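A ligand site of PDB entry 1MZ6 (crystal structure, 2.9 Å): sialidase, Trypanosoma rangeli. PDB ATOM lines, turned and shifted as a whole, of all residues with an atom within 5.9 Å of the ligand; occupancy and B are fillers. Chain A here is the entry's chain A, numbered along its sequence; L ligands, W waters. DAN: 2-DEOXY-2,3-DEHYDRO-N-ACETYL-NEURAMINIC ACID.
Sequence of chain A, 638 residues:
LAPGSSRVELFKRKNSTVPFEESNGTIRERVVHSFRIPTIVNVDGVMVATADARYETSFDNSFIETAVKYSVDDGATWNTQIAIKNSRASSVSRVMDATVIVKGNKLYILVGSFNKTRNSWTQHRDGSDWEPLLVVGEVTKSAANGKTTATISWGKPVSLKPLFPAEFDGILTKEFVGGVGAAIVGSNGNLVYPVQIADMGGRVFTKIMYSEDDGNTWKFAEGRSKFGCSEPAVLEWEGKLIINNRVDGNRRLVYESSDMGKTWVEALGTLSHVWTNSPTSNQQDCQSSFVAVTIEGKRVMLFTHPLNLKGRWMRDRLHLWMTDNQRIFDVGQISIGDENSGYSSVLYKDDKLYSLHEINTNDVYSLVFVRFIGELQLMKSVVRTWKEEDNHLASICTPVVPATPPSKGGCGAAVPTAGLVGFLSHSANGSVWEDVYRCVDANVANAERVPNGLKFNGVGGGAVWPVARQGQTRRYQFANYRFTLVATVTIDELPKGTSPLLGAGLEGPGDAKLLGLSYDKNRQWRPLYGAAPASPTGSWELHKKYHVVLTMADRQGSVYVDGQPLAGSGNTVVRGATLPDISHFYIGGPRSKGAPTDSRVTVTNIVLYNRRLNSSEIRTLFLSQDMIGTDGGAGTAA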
ATOM      1  N   ARG A  36      25.398  -8.276  31.097  1.00  0.00           N
ATOM      2  CA  ARG A  36      24.461  -7.645  30.170  1.00  0.00           C
ATOM      3  C   ARG A  36      24.384  -8.528  28.941  1.00  0.00           C
ATOM      4  O   ARG A  36      25.177  -9.441  28.835  1.00  0.00           O
ATOM      5  CB  ARG A  36      25.021  -6.301  29.727  1.00  0.00           C
ATOM      6  CG  ARG A  36      24.809  -5.120  30.690  1.00  0.00           C
ATOM      7  CD  ARG A  36      24.538  -3.765  30.014  1.00  0.00           C
ATOM      8  NE  ARG A  36      23.328  -3.874  29.216  1.00  0.00           N
ATOM      9  CZ  ARG A  36      22.983  -3.134  28.142  1.00  0.00           C
ATOM     10  NH1 ARG A  36      21.852  -3.407  27.521  1.00  0.00           N
ATOM     11  NH2 ARG A  36      23.721  -2.116  27.687  1.00  0.00           N
ATOM     12  N   ILE A  37      23.445  -8.267  28.020  1.00  0.00           N
ATOM     13  CA  ILE A  37      23.312  -8.962  26.748  1.00  0.00           C
ATOM     14  C   ILE A  37      23.112 -10.454  26.789  1.00  0.00           C
ATOM     15  O   ILE A  37      23.805 -11.208  26.128  1.00  0.00           O
ATOM     16  CB  ILE A  37      24.478  -8.652  25.794  1.00  0.00           C
ATOM     17  CG1 ILE A  37      24.984  -7.198  25.921  1.00  0.00           C
ATOM     18  CG2 ILE A  37      24.090  -8.921  24.360  1.00  0.00           C
ATOM     19  CD1 ILE A  37      23.913  -6.138  25.903  1.00  0.00           C
ATOM     20  N   ASP A  52      27.459 -10.982  28.365  1.00  0.00           N
ATOM     21  CA  ASP A  52      28.642 -10.132  28.462  1.00  0.00           C
ATOM     22  C   ASP A  52      29.015 -10.125  29.910  1.00  0.00           C
ATOM     23  O   ASP A  52      28.211  -9.736  30.759  1.00  0.00           O
ATOM     24  CB  ASP A  52      28.369  -8.656  28.138  1.00  0.00           C
ATOM     25  CG  ASP A  52      28.574  -8.267  26.651  1.00  0.00           C
ATOM     26  OD1 ASP A  52      28.614  -9.105  25.714  1.00  0.00           O
ATOM     27  OD2 ASP A  52      28.667  -7.053  26.365  1.00  0.00           O
ATOM     28  N   ARG A  54      30.911  -8.105  32.096  1.00  0.00           N
ATOM     29  CA  ARG A  54      31.667  -6.859  32.043  1.00  0.00           C
ATOM     30  C   ARG A  54      32.297  -6.671  33.410  1.00  0.00           C
ATOM     31  O   ARG A  54      31.669  -6.209  34.394  1.00  0.00           O
ATOM     32  CB  ARG A  54      30.827  -5.657  31.605  1.00  0.00           C
ATOM     33  CG  ARG A  54      29.721  -5.875  30.604  1.00  0.00           C
ATOM     34  CD  ARG A  54      29.310  -4.598  29.815  1.00  0.00           C
ATOM     35  NE  ARG A  54      28.705  -4.934  28.511  1.00  0.00           N
ATOM     36  CZ  ARG A  54      28.090  -4.066  27.746  1.00  0.00           C
ATOM     37  NH1 ARG A  54      27.989  -2.802  28.134  1.00  0.00           N
ATOM     38  NH2 ARG A  54      27.571  -4.442  26.586  1.00  0.00           N
ATOM     39  N   ASP A  60      29.826  -0.160  27.680  1.00  0.00           N
ATOM     40  CA  ASP A  60      30.201  -0.838  26.458  1.00  0.00           C
ATOM     41  C   ASP A  60      31.701  -0.937  26.178  1.00  0.00           C
ATOM     42  O   ASP A  60      32.223  -2.011  25.819  1.00  0.00           O
ATOM     43  CB  ASP A  60      29.609  -0.073  25.299  1.00  0.00           C
ATOM     44  CG  ASP A  60      28.120  -0.223  25.183  1.00  0.00           C
ATOM     45  OD1 ASP A  60      27.610   0.309  24.183  1.00  0.00           O
ATOM     46  OD2 ASP A  60      27.359  -0.832  25.959  1.00  0.00           O
ATOM     47  N   ASN A  61      32.400   0.197  26.260  1.00  0.00           N
ATOM     48  CA  ASN A  61      33.820   0.193  25.905  1.00  0.00           C
ATOM     49  C   ASN A  61      34.746  -0.056  27.040  1.00  0.00           C
ATOM     50  O   ASN A  61      35.712   0.666  27.163  1.00  0.00           O
ATOM     51  CB  ASN A  61      34.253   1.511  25.284  1.00  0.00           C
ATOM     52  CG  ASN A  61      33.187   2.113  24.406  1.00  0.00           C
ATOM     53  OD1 ASN A  61      33.109   1.848  23.205  1.00  0.00           O
ATOM     54  ND2 ASN A  61      32.352   2.937  25.021  1.00  0.00           N
ATOM     55  N   MET A  96      31.930  -8.883  22.713  1.00  0.00           N
ATOM     56  CA  MET A  96      30.596  -8.569  23.177  1.00  0.00           C
ATOM     57  C   MET A  96      29.518  -8.895  22.151  1.00  0.00           C
ATOM     58  O   MET A  96      29.790  -9.281  21.004  1.00  0.00           O
ATOM     59  CB  MET A  96      30.563  -7.083  23.425  1.00  0.00           C
ATOM     60  CG  MET A  96      31.210  -6.257  22.277  1.00  0.00           C
ATOM     61  SD  MET A  96      31.592  -4.509  22.821  1.00  0.00           S
ATOM     62  CE  MET A  96      29.860  -4.118  23.403  1.00  0.00           C
ATOM     63  N   ASP A  97      28.277  -8.761  22.602  1.00  0.00           N
ATOM     64  CA  ASP A  97      27.120  -8.796  21.735  1.00  0.00           C
ATOM     65  C   ASP A  97      26.926 -10.135  21.032  1.00  0.00           C
ATOM     66  O   ASP A  97      26.704 -10.212  19.816  1.00  0.00           O
ATOM     67  CB  ASP A  97      27.220  -7.655  20.718  1.00  0.00           C
ATOM     68  CG  ASP A  97      27.099  -6.247  21.373  1.00  0.00           C
ATOM     69  OD1 ASP A  97      27.140  -6.066  22.628  1.00  0.00           O
ATOM     70  OD2 ASP A  97      26.928  -5.227  20.666  1.00  0.00           O
ATOM     71  N   PHE A 114      36.937  -6.015  19.988  1.00  0.00           N
ATOM     72  CA  PHE A 114      37.720  -4.805  19.890  1.00  0.00           C
ATOM     73  C   PHE A 114      38.864  -4.814  20.889  1.00  0.00           C
ATOM     74  O   PHE A 114      38.806  -5.449  21.952  1.00  0.00           O
ATOM     75  CB  PHE A 114      36.862  -3.578  20.103  1.00  0.00           C
ATOM     76  CG  PHE A 114      35.539  -3.588  19.362  1.00  0.00           C
ATOM     77  CD1 PHE A 114      34.432  -4.225  19.897  1.00  0.00           C
ATOM     78  CD2 PHE A 114      35.382  -2.901  18.152  1.00  0.00           C
ATOM     79  CE1 PHE A 114      33.209  -4.211  19.241  1.00  0.00           C
ATOM     80  CE2 PHE A 114      34.140  -2.874  17.488  1.00  0.00           C
ATOM     81  CZ  PHE A 114      33.059  -3.530  18.042  1.00  0.00           C
ATOM     82  N   SER A 120      32.341   4.331  20.729  1.00  0.00           N
ATOM     83  CA  SER A 120      31.513   3.280  20.162  1.00  0.00           C
ATOM     84  C   SER A 120      31.632   3.041  18.632  1.00  0.00           C
ATOM     85  O   SER A 120      31.977   3.945  17.841  1.00  0.00           O
ATOM     86  CB  SER A 120      30.058   3.492  20.561  1.00  0.00           C
ATOM     87  OG  SER A 120      29.536   4.543  19.792  1.00  0.00           O
ATOM     88  N   TRP A 121      31.277   1.812  18.240  1.00  0.00           N
ATOM     89  CA  TRP A 121      31.587   1.283  16.925  1.00  0.00           C
ATOM     90  C   TRP A 121      31.164   2.033  15.670  1.00  0.00           C
ATOM     91  O   TRP A 121      31.927   2.038  14.681  1.00  0.00           O
ATOM     92  CB  TRP A 121      31.226  -0.186  16.807  1.00  0.00           C
ATOM     93  CG  TRP A 121      29.793  -0.540  16.599  1.00  0.00           C
ATOM     94  CD1 TRP A 121      28.772  -0.370  17.466  1.00  0.00           C
ATOM     95  CD2 TRP A 121      29.243  -1.233  15.473  1.00  0.00           C
ATOM     96  NE1 TRP A 121      27.614  -0.884  16.950  1.00  0.00           N
ATOM     97  CE2 TRP A 121      27.877  -1.416  15.718  1.00  0.00           C
ATOM     98  CE3 TRP A 121      29.769  -1.701  14.279  1.00  0.00           C
ATOM     99  CZ2 TRP A 121      27.039  -2.039  14.826  1.00  0.00           C
ATOM    100  CZ3 TRP A 121      28.937  -2.326  13.374  1.00  0.00           C
ATOM    101  CH2 TRP A 121      27.583  -2.486  13.650  1.00  0.00           C
ATOM    102  N   THR A 122      30.007   2.668  15.674  1.00  0.00           N
ATOM    103  CA  THR A 122      29.617   3.318  14.447  1.00  0.00           C
ATOM    104  C   THR A 122      30.504   4.519  14.198  1.00  0.00           C
ATOM    105  O   THR A 122      30.742   4.916  13.048  1.00  0.00           O
ATOM    106  CB  THR A 122      28.148   3.652  14.480  1.00  0.00           C
ATOM    107  OG1 THR A 122      27.833   4.252  15.744  1.00  0.00           O
ATOM    108  CG2 THR A 122      27.345   2.376  14.521  1.00  0.00           C
ATOM    109  N   VAL A 177      28.545  -6.636  13.069  1.00  0.00           N
ATOM    110  CA  VAL A 177      28.313  -7.450  14.243  1.00  0.00           C
ATOM    111  C   VAL A 177      27.027  -8.234  13.999  1.00  0.00           C
ATOM    112  O   VAL A 177      26.171  -7.827  13.191  1.00  0.00           O
ATOM    113  CB  VAL A 177      28.189  -6.581  15.502  1.00  0.00           C
ATOM    114  CG1 VAL A 177      27.761  -7.400  16.652  1.00  0.00           C
ATOM    115  CG2 VAL A 177      29.502  -5.955  15.849  1.00  0.00           C
ATOM    116  N   GLN A 196      24.369  -6.527  11.738  1.00  0.00           N
ATOM    117  CA  GLN A 196      24.271  -5.081  11.535  1.00  0.00           C
ATOM    118  C   GLN A 196      25.622  -4.555  11.054  1.00  0.00           C
ATOM    119  O   GLN A 196      26.647  -4.862  11.632  1.00  0.00           O
ATOM    120  CB  GLN A 196      23.737  -4.369  12.793  1.00  0.00           C
ATOM    121  CG  GLN A 196      24.663  -4.414  13.993  1.00  0.00           C
ATOM    122  CD  GLN A 196      23.988  -4.445  15.367  1.00  0.00           C
ATOM    123  OE1 GLN A 196      24.257  -5.329  16.170  1.00  0.00           O
ATOM    124  NE2 GLN A 196      23.121  -3.467  15.633  1.00  0.00           N
ATOM    125  N   SER A 230      19.374  -1.368  13.212  1.00  0.00           N
ATOM    126  CA  SER A 230      20.489  -1.992  13.874  1.00  0.00           C
ATOM    127  C   SER A 230      19.945  -3.140  14.687  1.00  0.00           C
ATOM    128  O   SER A 230      18.724  -3.246  14.842  1.00  0.00           O
ATOM    129  CB  SER A 230      21.160  -0.973  14.779  1.00  0.00           C
ATOM    130  OG  SER A 230      20.171  -0.217  15.447  1.00  0.00           O
ATOM    131  N   GLU A 231      20.851  -3.987  15.189  1.00  0.00           N
ATOM    132  CA  GLU A 231      20.510  -5.172  15.982  1.00  0.00           C
ATOM    133  C   GLU A 231      19.303  -5.908  15.432  1.00  0.00           C
ATOM    134  O   GLU A 231      18.278  -5.925  16.061  1.00  0.00           O
ATOM    135  CB  GLU A 231      20.256  -4.792  17.478  1.00  0.00           C
ATOM    136  CG  GLU A 231      21.525  -4.642  18.314  1.00  0.00           C
ATOM    137  CD  GLU A 231      21.358  -4.056  19.740  1.00  0.00           C
ATOM    138  OE1 GLU A 231      20.264  -3.647  20.146  1.00  0.00           O
ATOM    139  OE2 GLU A 231      22.368  -4.004  20.490  1.00  0.00           O
ATOM    140  N   ARG A 246      15.945  -3.079  15.229  1.00  0.00           N
ATOM    141  CA  ARG A 246      15.964  -2.086  16.260  1.00  0.00           C
ATOM    142  C   ARG A 246      16.049  -0.773  15.484  1.00  0.00           C
ATOM    143  O   ARG A 246      16.786  -0.731  14.503  1.00  0.00           O
ATOM    144  CB  ARG A 246      17.209  -2.296  17.085  1.00  0.00           C
ATOM    145  CG  ARG A 246      17.585  -1.075  17.850  1.00  0.00           C
ATOM    146  CD  ARG A 246      18.183  -1.290  19.218  1.00  0.00           C
ATOM    147  NE  ARG A 246      18.518   0.040  19.646  1.00  0.00           N
ATOM    148  CZ  ARG A 246      19.491   0.401  20.493  1.00  0.00           C
ATOM    149  NH1 ARG A 246      20.287  -0.485  21.099  1.00  0.00           N
ATOM    150  NH2 ARG A 246      19.614   1.702  20.713  1.00  0.00           N
ATOM    151  N   ASP A 248      16.670   3.301  16.389  1.00  0.00           N
ATOM    152  CA  ASP A 248      16.765   4.434  17.287  1.00  0.00           C
ATOM    153  C   ASP A 248      16.002   5.648  16.762  1.00  0.00           C
ATOM    154  O   ASP A 248      16.159   6.064  15.617  1.00  0.00           O
ATOM    155  CB  ASP A 248      18.209   4.792  17.536  1.00  0.00           C
ATOM    156  CG  ASP A 248      18.922   3.756  18.364  1.00  0.00           C
ATOM    157  OD1 ASP A 248      20.139   3.517  18.112  1.00  0.00           O
ATOM    158  OD2 ASP A 248      18.330   3.139  19.301  1.00  0.00           O
ATOM    159  N   GLN A 284      15.965   6.113  22.451  1.00  0.00           N
ATOM    160  CA  GLN A 284      16.882   5.154  21.881  1.00  0.00           C
ATOM    161  C   GLN A 284      16.132   3.885  22.000  1.00  0.00           C
ATOM    162  O   GLN A 284      15.335   3.735  22.901  1.00  0.00           O
ATOM    163  CB  GLN A 284      18.225   5.149  22.547  1.00  0.00           C
ATOM    164  CG  GLN A 284      18.477   4.114  23.567  1.00  0.00           C
ATOM    165  CD  GLN A 284      19.579   4.600  24.478  1.00  0.00           C
ATOM    166  OE1 GLN A 284      19.331   5.526  25.271  1.00  0.00           O
ATOM    167  NE2 GLN A 284      20.800   4.065  24.328  1.00  0.00           N
ATOM    168  N   ASP A 285      16.308   2.999  21.045  1.00  0.00           N
ATOM    169  CA  ASP A 285      15.517   1.797  21.024  1.00  0.00           C
ATOM    170  C   ASP A 285      16.267   0.749  21.769  1.00  0.00           C
ATOM    171  O   ASP A 285      17.301   1.032  22.384  1.00  0.00           O
ATOM    172  CB  ASP A 285      15.210   1.361  19.601  1.00  0.00           C
ATOM    173  CG  ASP A 285      14.024   0.468  19.548  1.00  0.00           C
ATOM    174  OD1 ASP A 285      13.591   0.059  20.652  1.00  0.00           O
ATOM    175  OD2 ASP A 285      13.460   0.114  18.482  1.00  0.00           O
ATOM    176  N   ARG A 315      14.459   1.570  30.055  1.00  0.00           N
ATOM    177  CA  ARG A 315      13.918   0.325  29.592  1.00  0.00           C
ATOM    178  C   ARG A 315      13.168  -0.360  30.703  1.00  0.00           C
ATOM    179  O   ARG A 315      13.453  -1.478  31.079  1.00  0.00           O
ATOM    180  CB  ARG A 315      15.040  -0.527  29.009  1.00  0.00           C
ATOM    181  CG  ARG A 315      15.610   0.081  27.754  1.00  0.00           C
ATOM    182  CD  ARG A 315      17.001  -0.346  27.443  1.00  0.00           C
ATOM    183  NE  ARG A 315      17.589   0.291  26.273  1.00  0.00           N
ATOM    184  CZ  ARG A 315      18.853   0.060  25.876  1.00  0.00           C
ATOM    185  NH1 ARG A 315      19.589  -0.787  26.576  1.00  0.00           N
ATOM    186  NH2 ARG A 315      19.398   0.657  24.804  1.00  0.00           N
ATOM    187  N   TYR A 343      17.761  -5.657  27.579  1.00  0.00           N
ATOM    188  CA  TYR A 343      17.795  -6.723  26.578  1.00  0.00           C
ATOM    189  C   TYR A 343      17.279  -8.048  27.194  1.00  0.00           C
ATOM    190  O   TYR A 343      17.690  -8.386  28.264  1.00  0.00           O
ATOM    191  CB  TYR A 343      19.219  -6.923  26.105  1.00  0.00           C
ATOM    192  CG  TYR A 343      19.845  -5.890  25.173  1.00  0.00           C
ATOM    193  CD1 TYR A 343      19.427  -4.569  25.127  1.00  0.00           C
ATOM    194  CD2 TYR A 343      20.887  -6.254  24.369  1.00  0.00           C
ATOM    195  CE1 TYR A 343      20.040  -3.647  24.285  1.00  0.00           C
ATOM    196  CE2 TYR A 343      21.502  -5.353  23.523  1.00  0.00           C
ATOM    197  CZ  TYR A 343      21.091  -4.051  23.482  1.00  0.00           C
ATOM    198  OH  TYR A 343      21.710  -3.200  22.609  1.00  0.00           O
HETATM  199  C1  DAN L   1      22.673  -0.670  24.132  1.00  0.00           C
HETATM  200  C2  DAN L   1      23.752  -1.236  23.457  1.00  0.00           C
HETATM  201  C3  DAN L   1      24.407  -2.461  23.991  1.00  0.00           C
HETATM  202  C4  DAN L   1      25.483  -2.925  23.024  1.00  0.00           C
HETATM  203  C5  DAN L   1      26.156  -1.774  22.304  1.00  0.00           C
HETATM  204  C6  DAN L   1      25.045  -1.174  21.471  1.00  0.00           C
HETATM  205  C7  DAN L   1      25.527  -0.059  20.536  1.00  0.00           C
HETATM  206  C8  DAN L   1      24.432   0.865  19.983  1.00  0.00           C
HETATM  207  C9  DAN L   1      24.642   1.753  18.751  1.00  0.00           C
HETATM  208  C10 DAN L   1      28.260  -1.723  21.000  1.00  0.00           C
HETATM  209  C11 DAN L   1      29.166  -2.452  20.061  1.00  0.00           C
HETATM  210  N5  DAN L   1      27.283  -2.376  21.599  1.00  0.00           N
HETATM  211  O1A DAN L   1      22.183  -1.005  25.409  1.00  0.00           O
HETATM  212  O1B DAN L   1      22.087   0.293  23.513  1.00  0.00           O
HETATM  213  O4  DAN L   1      26.429  -3.677  23.739  1.00  0.00           O
HETATM  214  O6  DAN L   1      24.120  -0.627  22.403  1.00  0.00           O
HETATM  215  O7  DAN L   1      26.305   0.667  21.435  1.00  0.00           O
HETATM  216  O8  DAN L   1      23.318   0.093  19.700  1.00  0.00           O
HETATM  217  O9  DAN L   1      25.905   1.776  18.137  1.00  0.00           O
HETATM  218  O10 DAN L   1      28.426  -0.368  21.211  1.00  0.00           O
HETATM  219  O   HOH W   1      23.904   1.440  15.981  1.00  0.00           O
HETATM  220  O   HOH W   2      31.027   0.006  20.863  1.00  0.00           O
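The backbone NH (N) of Asp 97 lies within hydrogen-bond range of the side-chain carboxylate (OD1) of Asp 52, 3.1 Å away. The guanidinium group of Arg 315 sits at hydrogen-bond distance from the backbone carbonyl oxygen of Asp 285 (3.2 Å). NH1 of Arg 246 lies within hydrogen-bond range of OH of Tyr 343. The guanidinium group (NH1) of Arg 54 lies within salt-bridge range of the side-chain carboxylate (OD2) of Asp 60 (3.0 Å). The side-chain carboxylate (OE1) of Glu 231 is in salt-bridge range of the guanidinium group (NH1) of Arg 246 (3.3 Å). The guanidinium group of Arg 246 is in hydrogen-bond range of the backbone carbonyl oxygen of Asp 285 (2.9 Å). The backbone NH (N) of Arg 246 is in hydrogen-bond range of the backbone carbonyl oxygen (O) of Ser 230. OD2 of Asp 52 is in salt-bridge range of NH2 of Arg 54, at 2.8 Å.
An oxygen (O4) of the ligand is in hydrogen-bond range of the side-chain carboxylate (OD1) of Asp 97, at 2.7 Å. NH1 of Arg 315 is in salt-bridge range of O1A of the ligand (2.9 Å). An oxygen (O1A) of the ligand lies within salt-bridge range of the guanidinium group of Arg 36 (3.0 Å). OD1 of Asp 60 is in hydrogen-bond range of O7 of the ligand (3.1 Å). NH1 of Arg 246 is in salt-bridge range of O1B of the ligand. NH2 of Arg 54 sits at hydrogen-bond distance from O4 of the ligand, 3.2 Å away. The indole nitrogen (NE1) of Trp 121 sits at hydrogen-bond distance from an oxygen (O9) of the ligand (3.4 Å).
Merely in contact with the ligand: Met 96 (3.5 Å), Thr 122 (3.9 Å) and Tyr 343 (3.0 Å). Hydrophobic or aromatic side chains within 4 Å of the ligand: Met 96, Trp 121 and Tyr 343. Of the 22 residues printed, 10 come within 4 Å of the ligand. The nearest printed residue that does not touch the ligand is Glu 231 (4.02 Å).
Water W2 lies within hydrogen-bond range of O10 of the ligand (2.7 Å) and N of Trp 121 (3.2 Å).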
